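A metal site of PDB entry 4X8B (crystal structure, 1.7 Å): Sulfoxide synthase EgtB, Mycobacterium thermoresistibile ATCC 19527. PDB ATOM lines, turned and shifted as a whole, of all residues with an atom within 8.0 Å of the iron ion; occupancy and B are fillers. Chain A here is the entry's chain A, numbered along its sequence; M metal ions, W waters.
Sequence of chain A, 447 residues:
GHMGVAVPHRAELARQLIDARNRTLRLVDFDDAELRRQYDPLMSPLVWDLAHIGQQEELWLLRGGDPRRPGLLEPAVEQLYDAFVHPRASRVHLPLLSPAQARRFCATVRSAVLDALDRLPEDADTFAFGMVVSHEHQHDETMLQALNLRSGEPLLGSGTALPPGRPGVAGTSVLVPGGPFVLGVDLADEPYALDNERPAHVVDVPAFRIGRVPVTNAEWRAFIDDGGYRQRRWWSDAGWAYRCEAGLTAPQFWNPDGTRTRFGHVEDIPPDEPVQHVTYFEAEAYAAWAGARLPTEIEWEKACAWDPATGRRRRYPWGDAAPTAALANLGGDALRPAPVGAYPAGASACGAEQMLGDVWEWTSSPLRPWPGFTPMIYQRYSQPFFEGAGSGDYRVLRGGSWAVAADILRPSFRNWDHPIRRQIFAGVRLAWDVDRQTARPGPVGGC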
ATOM      1  N   TRP A  48      22.402 -16.097 -16.717  1.00  0.00           N
ATOM      2  CA  TRP A  48      22.000 -14.705 -16.600  1.00  0.00           C
ATOM      3  C   TRP A  48      20.780 -14.461 -17.494  1.00  0.00           C
ATOM      4  O   TRP A  48      19.786 -13.886 -17.054  1.00  0.00           O
ATOM      5  CB  TRP A  48      23.135 -13.761 -16.958  1.00  0.00           C
ATOM      6  CG  TRP A  48      22.777 -12.294 -16.740  1.00  0.00           C
ATOM      7  CD1 TRP A  48      23.061 -11.551 -15.632  1.00  0.00           C
ATOM      8  CD2 TRP A  48      22.106 -11.416 -17.660  1.00  0.00           C
ATOM      9  NE1 TRP A  48      22.606 -10.262 -15.802  1.00  0.00           N
ATOM     10  CE2 TRP A  48      21.977 -10.162 -17.013  1.00  0.00           C
ATOM     11  CE3 TRP A  48      21.574 -11.563 -18.942  1.00  0.00           C
ATOM     12  CZ2 TRP A  48      21.374  -9.073 -17.626  1.00  0.00           C
ATOM     13  CZ3 TRP A  48      20.932 -10.474 -19.543  1.00  0.00           C
ATOM     14  CH2 TRP A  48      20.836  -9.251 -18.868  1.00  0.00           C
ATOM     15  N   ASP A  49      20.849 -14.907 -18.749  1.00  0.00           N
ATOM     16  CA  ASP A  49      19.712 -14.747 -19.641  1.00  0.00           C
ATOM     17  C   ASP A  49      18.484 -15.453 -19.106  1.00  0.00           C
ATOM     18  O   ASP A  49      17.367 -14.902 -19.209  1.00  0.00           O
ATOM     19  CB  ASP A  49      20.020 -15.247 -21.057  1.00  0.00           C
ATOM     20  CG  ASP A  49      21.030 -14.355 -21.742  1.00  0.00           C
ATOM     21  OD1 ASP A  49      20.655 -13.339 -22.353  1.00  0.00           O
ATOM     22  OD2 ASP A  49      22.229 -14.662 -21.638  1.00  0.00           O
ATOM     23  N   HIS A  52      17.061 -13.313 -16.320  1.00  0.00           N
ATOM     24  CA  HIS A  52      16.676 -12.045 -16.904  1.00  0.00           C
ATOM     25  C   HIS A  52      15.342 -12.195 -17.666  1.00  0.00           C
ATOM     26  O   HIS A  52      14.466 -11.337 -17.599  1.00  0.00           O
ATOM     27  CB  HIS A  52      17.768 -11.526 -17.838  1.00  0.00           C
ATOM     28  CG  HIS A  52      17.359 -10.383 -18.716  1.00  0.00           C
ATOM     29  ND1 HIS A  52      17.426  -9.073 -18.318  1.00  0.00           N
ATOM     30  CD2 HIS A  52      16.956 -10.359 -20.014  1.00  0.00           C
ATOM     31  CE1 HIS A  52      17.044  -8.277 -19.315  1.00  0.00           C
ATOM     32  NE2 HIS A  52      16.763  -9.041 -20.357  1.00  0.00           N
ATOM     33  N   ILE A  53      15.195 -13.306 -18.385  1.00  0.00           N
ATOM     34  CA  ILE A  53      13.947 -13.584 -19.100  1.00  0.00           C
ATOM     35  C   ILE A  53      12.759 -13.594 -18.113  1.00  0.00           C
ATOM     36  O   ILE A  53      11.746 -12.888 -18.314  1.00  0.00           O
ATOM     37  CB  ILE A  53      14.059 -14.936 -19.856  1.00  0.00           C
ATOM     38  CG1 ILE A  53      14.886 -14.751 -21.135  1.00  0.00           C
ATOM     39  CG2 ILE A  53      12.683 -15.479 -20.228  1.00  0.00           C
ATOM     40  CD1 ILE A  53      15.366 -16.090 -21.710  1.00  0.00           C
ATOM     41  N   GLN A  55      12.675 -12.254 -15.072  1.00  0.00           N
ATOM     42  CA  GLN A  55      12.554 -10.976 -14.400  1.00  0.00           C
ATOM     43  C   GLN A  55      11.825  -9.961 -15.291  1.00  0.00           C
ATOM     44  O   GLN A  55      10.991  -9.180 -14.823  1.00  0.00           O
ATOM     45  CB  GLN A  55      13.948 -10.460 -14.017  1.00  0.00           C
ATOM     46  CG  GLN A  55      13.974  -9.144 -13.219  1.00  0.00           C
ATOM     47  CD  GLN A  55      13.921  -7.893 -14.089  1.00  0.00           C
ATOM     48  OE1 GLN A  55      14.370  -7.878 -15.231  1.00  0.00           O
ATOM     49  NE2 GLN A  55      13.358  -6.827 -13.530  1.00  0.00           N
ATOM     50  N   GLN A  56      12.126  -9.993 -16.581  1.00  0.00           N
ATOM     51  CA  GLN A  56      11.470  -9.088 -17.512  1.00  0.00           C
ATOM     52  C   GLN A  56       9.992  -9.499 -17.693  1.00  0.00           C
ATOM     53  O   GLN A  56       9.109  -8.643 -17.773  1.00  0.00           O
ATOM     54  CB  GLN A  56      12.223  -9.081 -18.842  1.00  0.00           C
ATOM     55  CG  GLN A  56      13.576  -8.413 -18.692  1.00  0.00           C
ATOM     56  CD  GLN A  56      13.457  -6.916 -18.714  1.00  0.00           C
ATOM     57  OE1 GLN A  56      13.144  -6.350 -19.750  1.00  0.00           O
ATOM     58  NE2 GLN A  56      13.679  -6.272 -17.579  1.00  0.00           N
ATOM     59  N   TRP A  60       7.020  -6.786 -16.861  1.00  0.00           N
ATOM     60  CA  TRP A  60       6.118  -6.213 -17.858  1.00  0.00           C
ATOM     61  C   TRP A  60       4.705  -6.785 -17.762  1.00  0.00           C
ATOM     62  O   TRP A  60       3.753  -6.112 -18.151  1.00  0.00           O
ATOM     63  CB  TRP A  60       6.667  -6.419 -19.286  1.00  0.00           C
ATOM     64  CG  TRP A  60       8.052  -5.870 -19.457  1.00  0.00           C
ATOM     65  CD1 TRP A  60       9.160  -6.572 -19.836  1.00  0.00           C
ATOM     66  CD2 TRP A  60       8.475  -4.523 -19.242  1.00  0.00           C
ATOM     67  NE1 TRP A  60      10.253  -5.743 -19.863  1.00  0.00           N
ATOM     68  CE2 TRP A  60       9.869  -4.487 -19.494  1.00  0.00           C
ATOM     69  CE3 TRP A  60       7.836  -3.347 -18.842  1.00  0.00           C
ATOM     70  CZ2 TRP A  60      10.623  -3.320 -19.358  1.00  0.00           C
ATOM     71  CZ3 TRP A  60       8.581  -2.181 -18.711  1.00  0.00           C
ATOM     72  CH2 TRP A  60       9.968  -2.188 -18.962  1.00  0.00           C
ATOM     73  N   TYR A  81      20.004  -8.162 -13.044  1.00  0.00           N
ATOM     74  CA  TYR A  81      19.502  -8.520 -14.378  1.00  0.00           C
ATOM     75  C   TYR A  81      19.120  -7.294 -15.211  1.00  0.00           C
ATOM     76  O   TYR A  81      18.460  -7.404 -16.259  1.00  0.00           O
ATOM     77  CB  TYR A  81      18.344  -9.514 -14.216  1.00  0.00           C
ATOM     78  CG  TYR A  81      18.836 -10.720 -13.473  1.00  0.00           C
ATOM     79  CD1 TYR A  81      19.669 -11.646 -14.102  1.00  0.00           C
ATOM     80  CD2 TYR A  81      18.543 -10.895 -12.127  1.00  0.00           C
ATOM     81  CE1 TYR A  81      20.207 -12.720 -13.404  1.00  0.00           C
ATOM     82  CE2 TYR A  81      19.055 -11.990 -11.417  1.00  0.00           C
ATOM     83  CZ  TYR A  81      19.879 -12.898 -12.075  1.00  0.00           C
ATOM     84  OH  TYR A  81      20.342 -13.979 -11.359  1.00  0.00           O
ATOM     85  N   ALA A  83      20.225  -4.861 -17.743  1.00  0.00           N
ATOM     86  CA  ALA A  83      21.271  -4.855 -18.737  1.00  0.00           C
ATOM     87  C   ALA A  83      21.987  -3.529 -18.842  1.00  0.00           C
ATOM     88  O   ALA A  83      23.131  -3.484 -19.291  1.00  0.00           O
ATOM     89  CB  ALA A  83      20.692  -5.226 -20.116  1.00  0.00           C
ATOM     90  N   ARG A  88      28.049  -6.621 -20.317  1.00  0.00           N
ATOM     91  CA  ARG A  88      28.093  -8.056 -20.584  1.00  0.00           C
ATOM     92  C   ARG A  88      29.255  -8.804 -19.932  1.00  0.00           C
ATOM     93  O   ARG A  88      29.058  -9.851 -19.310  1.00  0.00           O
ATOM     94  CB  ARG A  88      28.153  -8.302 -22.100  1.00  0.00           C
ATOM     95  CG  ARG A  88      26.866  -7.992 -22.820  1.00  0.00           C
ATOM     96  CD  ARG A  88      26.017  -9.248 -22.978  1.00  0.00           C
ATOM     97  NE  ARG A  88      24.793  -9.034 -23.745  1.00  0.00           N
ATOM     98  CZ  ARG A  88      24.621  -9.352 -25.029  1.00  0.00           C
ATOM     99  NH1 ARG A  88      25.599  -9.880 -25.759  1.00  0.00           N
ATOM    100  NH2 ARG A  88      23.453  -9.129 -25.593  1.00  0.00           N
ATOM    101  N   ARG A  91      29.173  -9.868 -16.157  1.00  0.00           N
ATOM    102  CA  ARG A  91      28.054 -10.613 -15.612  1.00  0.00           C
ATOM    103  C   ARG A  91      28.456 -11.985 -15.072  1.00  0.00           C
ATOM    104  O   ARG A  91      27.841 -12.487 -14.133  1.00  0.00           O
ATOM    105  CB  ARG A  91      26.942 -10.741 -16.670  1.00  0.00           C
ATOM    106  CG  ARG A  91      26.315  -9.385 -16.979  1.00  0.00           C
ATOM    107  CD  ARG A  91      25.324  -9.456 -18.133  1.00  0.00           C
ATOM    108  NE  ARG A  91      24.993  -8.102 -18.588  1.00  0.00           N
ATOM    109  CZ  ARG A  91      24.253  -7.838 -19.641  1.00  0.00           C
ATOM    110  NH1 ARG A  91      23.710  -8.827 -20.347  1.00  0.00           N
ATOM    111  NH2 ARG A  91      24.054  -6.556 -19.992  1.00  0.00           N
ATOM    112  N   HIS A 135      10.597 -10.545 -26.538  1.00  0.00           N
ATOM    113  CA  HIS A 135      11.759 -10.458 -25.666  1.00  0.00           C
ATOM    114  C   HIS A 135      12.417 -11.820 -25.420  1.00  0.00           C
ATOM    115  O   HIS A 135      13.634 -11.963 -25.512  1.00  0.00           O
ATOM    116  CB  HIS A 135      11.377  -9.803 -24.326  1.00  0.00           C
ATOM    117  CG  HIS A 135      12.548  -9.620 -23.418  1.00  0.00           C
ATOM    118  ND1 HIS A 135      12.808 -10.454 -22.351  1.00  0.00           N
ATOM    119  CD2 HIS A 135      13.577  -8.739 -23.482  1.00  0.00           C
ATOM    120  CE1 HIS A 135      13.958 -10.094 -21.789  1.00  0.00           C
ATOM    121  NE2 HIS A 135      14.445  -9.060 -22.455  1.00  0.00           N
ATOM    122  N   GLU A 136      11.618 -12.826 -25.102  1.00  0.00           N
ATOM    123  CA  GLU A 136      12.191 -14.123 -24.761  1.00  0.00           C
ATOM    124  C   GLU A 136      12.848 -14.759 -25.982  1.00  0.00           C
ATOM    125  O   GLU A 136      13.976 -15.242 -25.912  1.00  0.00           O
ATOM    126  CB  GLU A 136      11.126 -15.054 -24.163  1.00  0.00           C
ATOM    127  CG  GLU A 136      11.734 -16.429 -23.766  1.00  0.00           C
ATOM    128  CD  GLU A 136      10.989 -17.206 -22.706  1.00  0.00           C
ATOM    129  OE1 GLU A 136       9.892 -16.781 -22.263  1.00  0.00           O
ATOM    130  OE2 GLU A 136      11.535 -18.261 -22.299  1.00  0.00           O
ATOM    131  N   GLN A 138      14.093 -13.250 -28.529  1.00  0.00           N
ATOM    132  CA  GLN A 138      15.319 -12.503 -28.815  1.00  0.00           C
ATOM    133  C   GLN A 138      16.483 -12.970 -27.935  1.00  0.00           C
ATOM    134  O   GLN A 138      17.608 -13.127 -28.406  1.00  0.00           O
ATOM    135  CB  GLN A 138      15.121 -10.994 -28.632  1.00  0.00           C
ATOM    136  CG  GLN A 138      14.229 -10.402 -29.721  1.00  0.00           C
ATOM    137  CD  GLN A 138      14.162  -8.906 -29.622  1.00  0.00           C
ATOM    138  OE1 GLN A 138      15.205  -8.261 -29.498  1.00  0.00           O
ATOM    139  NE2 GLN A 138      12.951  -8.330 -29.672  1.00  0.00           N
ATOM    140  N   HIS A 139      16.218 -13.216 -26.656  1.00  0.00           N
ATOM    141  CA  HIS A 139      17.243 -13.780 -25.796  1.00  0.00           C
ATOM    142  C   HIS A 139      17.588 -15.215 -26.175  1.00  0.00           C
ATOM    143  O   HIS A 139      18.718 -15.651 -25.934  1.00  0.00           O
ATOM    144  CB  HIS A 139      16.827 -13.665 -24.310  1.00  0.00           C
ATOM    145  CG  HIS A 139      17.111 -12.319 -23.744  1.00  0.00           C
ATOM    146  ND1 HIS A 139      18.352 -11.977 -23.229  1.00  0.00           N
ATOM    147  CD2 HIS A 139      16.350 -11.193 -23.654  1.00  0.00           C
ATOM    148  CE1 HIS A 139      18.346 -10.706 -22.856  1.00  0.00           C
ATOM    149  NE2 HIS A 139      17.139 -10.202 -23.110  1.00  0.00           N
ATOM    150  N   THR A 142      20.171 -14.677 -28.667  1.00  0.00           N
ATOM    151  CA  THR A 142      21.389 -14.279 -27.955  1.00  0.00           C
ATOM    152  C   THR A 142      22.113 -15.501 -27.341  1.00  0.00           C
ATOM    153  O   THR A 142      23.330 -15.639 -27.458  1.00  0.00           O
ATOM    154  CB  THR A 142      21.043 -13.265 -26.854  1.00  0.00           C
ATOM    155  OG1 THR A 142      20.488 -12.079 -27.444  1.00  0.00           O
ATOM    156  CG2 THR A 142      22.287 -12.859 -26.083  1.00  0.00           C
ATOM    157  N   TYR A 378       7.958  -0.740 -22.286  1.00  0.00           N
ATOM    158  CA  TYR A 378       9.404  -0.895 -22.137  1.00  0.00           C
ATOM    159  C   TYR A 378      10.076   0.295 -22.838  1.00  0.00           C
ATOM    160  O   TYR A 378      10.497   0.222 -24.001  1.00  0.00           O
ATOM    161  CB  TYR A 378       9.817  -2.245 -22.736  1.00  0.00           C
ATOM    162  CG  TYR A 378      11.254  -2.686 -22.595  1.00  0.00           C
ATOM    163  CD1 TYR A 378      12.225  -1.868 -22.032  1.00  0.00           C
ATOM    164  CD2 TYR A 378      11.633  -3.955 -23.021  1.00  0.00           C
ATOM    165  CE1 TYR A 378      13.526  -2.299 -21.912  1.00  0.00           C
ATOM    166  CE2 TYR A 378      12.934  -4.386 -22.901  1.00  0.00           C
ATOM    167  CZ  TYR A 378      13.874  -3.562 -22.346  1.00  0.00           C
ATOM    168  OH  TYR A 378      15.172  -4.000 -22.219  1.00  0.00           O
ATOM    169  N   TYR A 381      13.627   0.291 -24.517  1.00  0.00           N
ATOM    170  CA  TYR A 381      13.940  -0.712 -25.508  1.00  0.00           C
ATOM    171  C   TYR A 381      14.608  -0.113 -26.748  1.00  0.00           C
ATOM    172  O   TYR A 381      15.617  -0.656 -27.223  1.00  0.00           O
ATOM    173  CB  TYR A 381      12.673  -1.490 -25.906  1.00  0.00           C
ATOM    174  CG  TYR A 381      12.911  -2.530 -26.963  1.00  0.00           C
ATOM    175  CD1 TYR A 381      13.414  -3.788 -26.646  1.00  0.00           C
ATOM    176  CD2 TYR A 381      12.634  -2.265 -28.301  1.00  0.00           C
ATOM    177  CE1 TYR A 381      13.649  -4.753 -27.664  1.00  0.00           C
ATOM    178  CE2 TYR A 381      12.847  -3.214 -29.300  1.00  0.00           C
ATOM    179  CZ  TYR A 381      13.344  -4.443 -28.973  1.00  0.00           C
ATOM    180  OH  TYR A 381      13.572  -5.350 -29.985  1.00  0.00           O
HETATM  181 FE    FE M   1      16.402  -8.372 -22.355  1.00  0.00          FE
HETATM  182  O   HOH W   1      18.265  -7.433 -22.421  1.00  0.00           O
HETATM  183  O   HOH W   2      16.237  -7.462 -24.334  1.00  0.00           O
HETATM  184  O   HOH W   3      15.580  -6.435 -21.581  1.00  0.00           O
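Water W3 bridges OH of Tyr 378 (2.6 Å) and OE1 of Gln 56 (3.0 Å).
A ring nitrogen (ND1) of His 52 lies within hydrogen-bond range of the backbone carbonyl oxygen (O) of Tyr 81, 2.8 Å away. The side-chain carboxylate of Asp 49 sits at hydrogen-bond distance from a ring nitrogen (ND1) of His 139, 2.8 Å away.
The iron ion is bound by a ring nitrogen (NE2) of His 135, water W1, a ring nitrogen (NE2) of His 139, a ring nitrogen (NE2) of His 52, water W2 and water W3. The iron ion has six donor atoms within binding distance.
Within 4 Å of the iron ion: His 52, His 135 and His 139. Along chain A the residues within 4 Å of the iron ion span positions 52 to 139.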
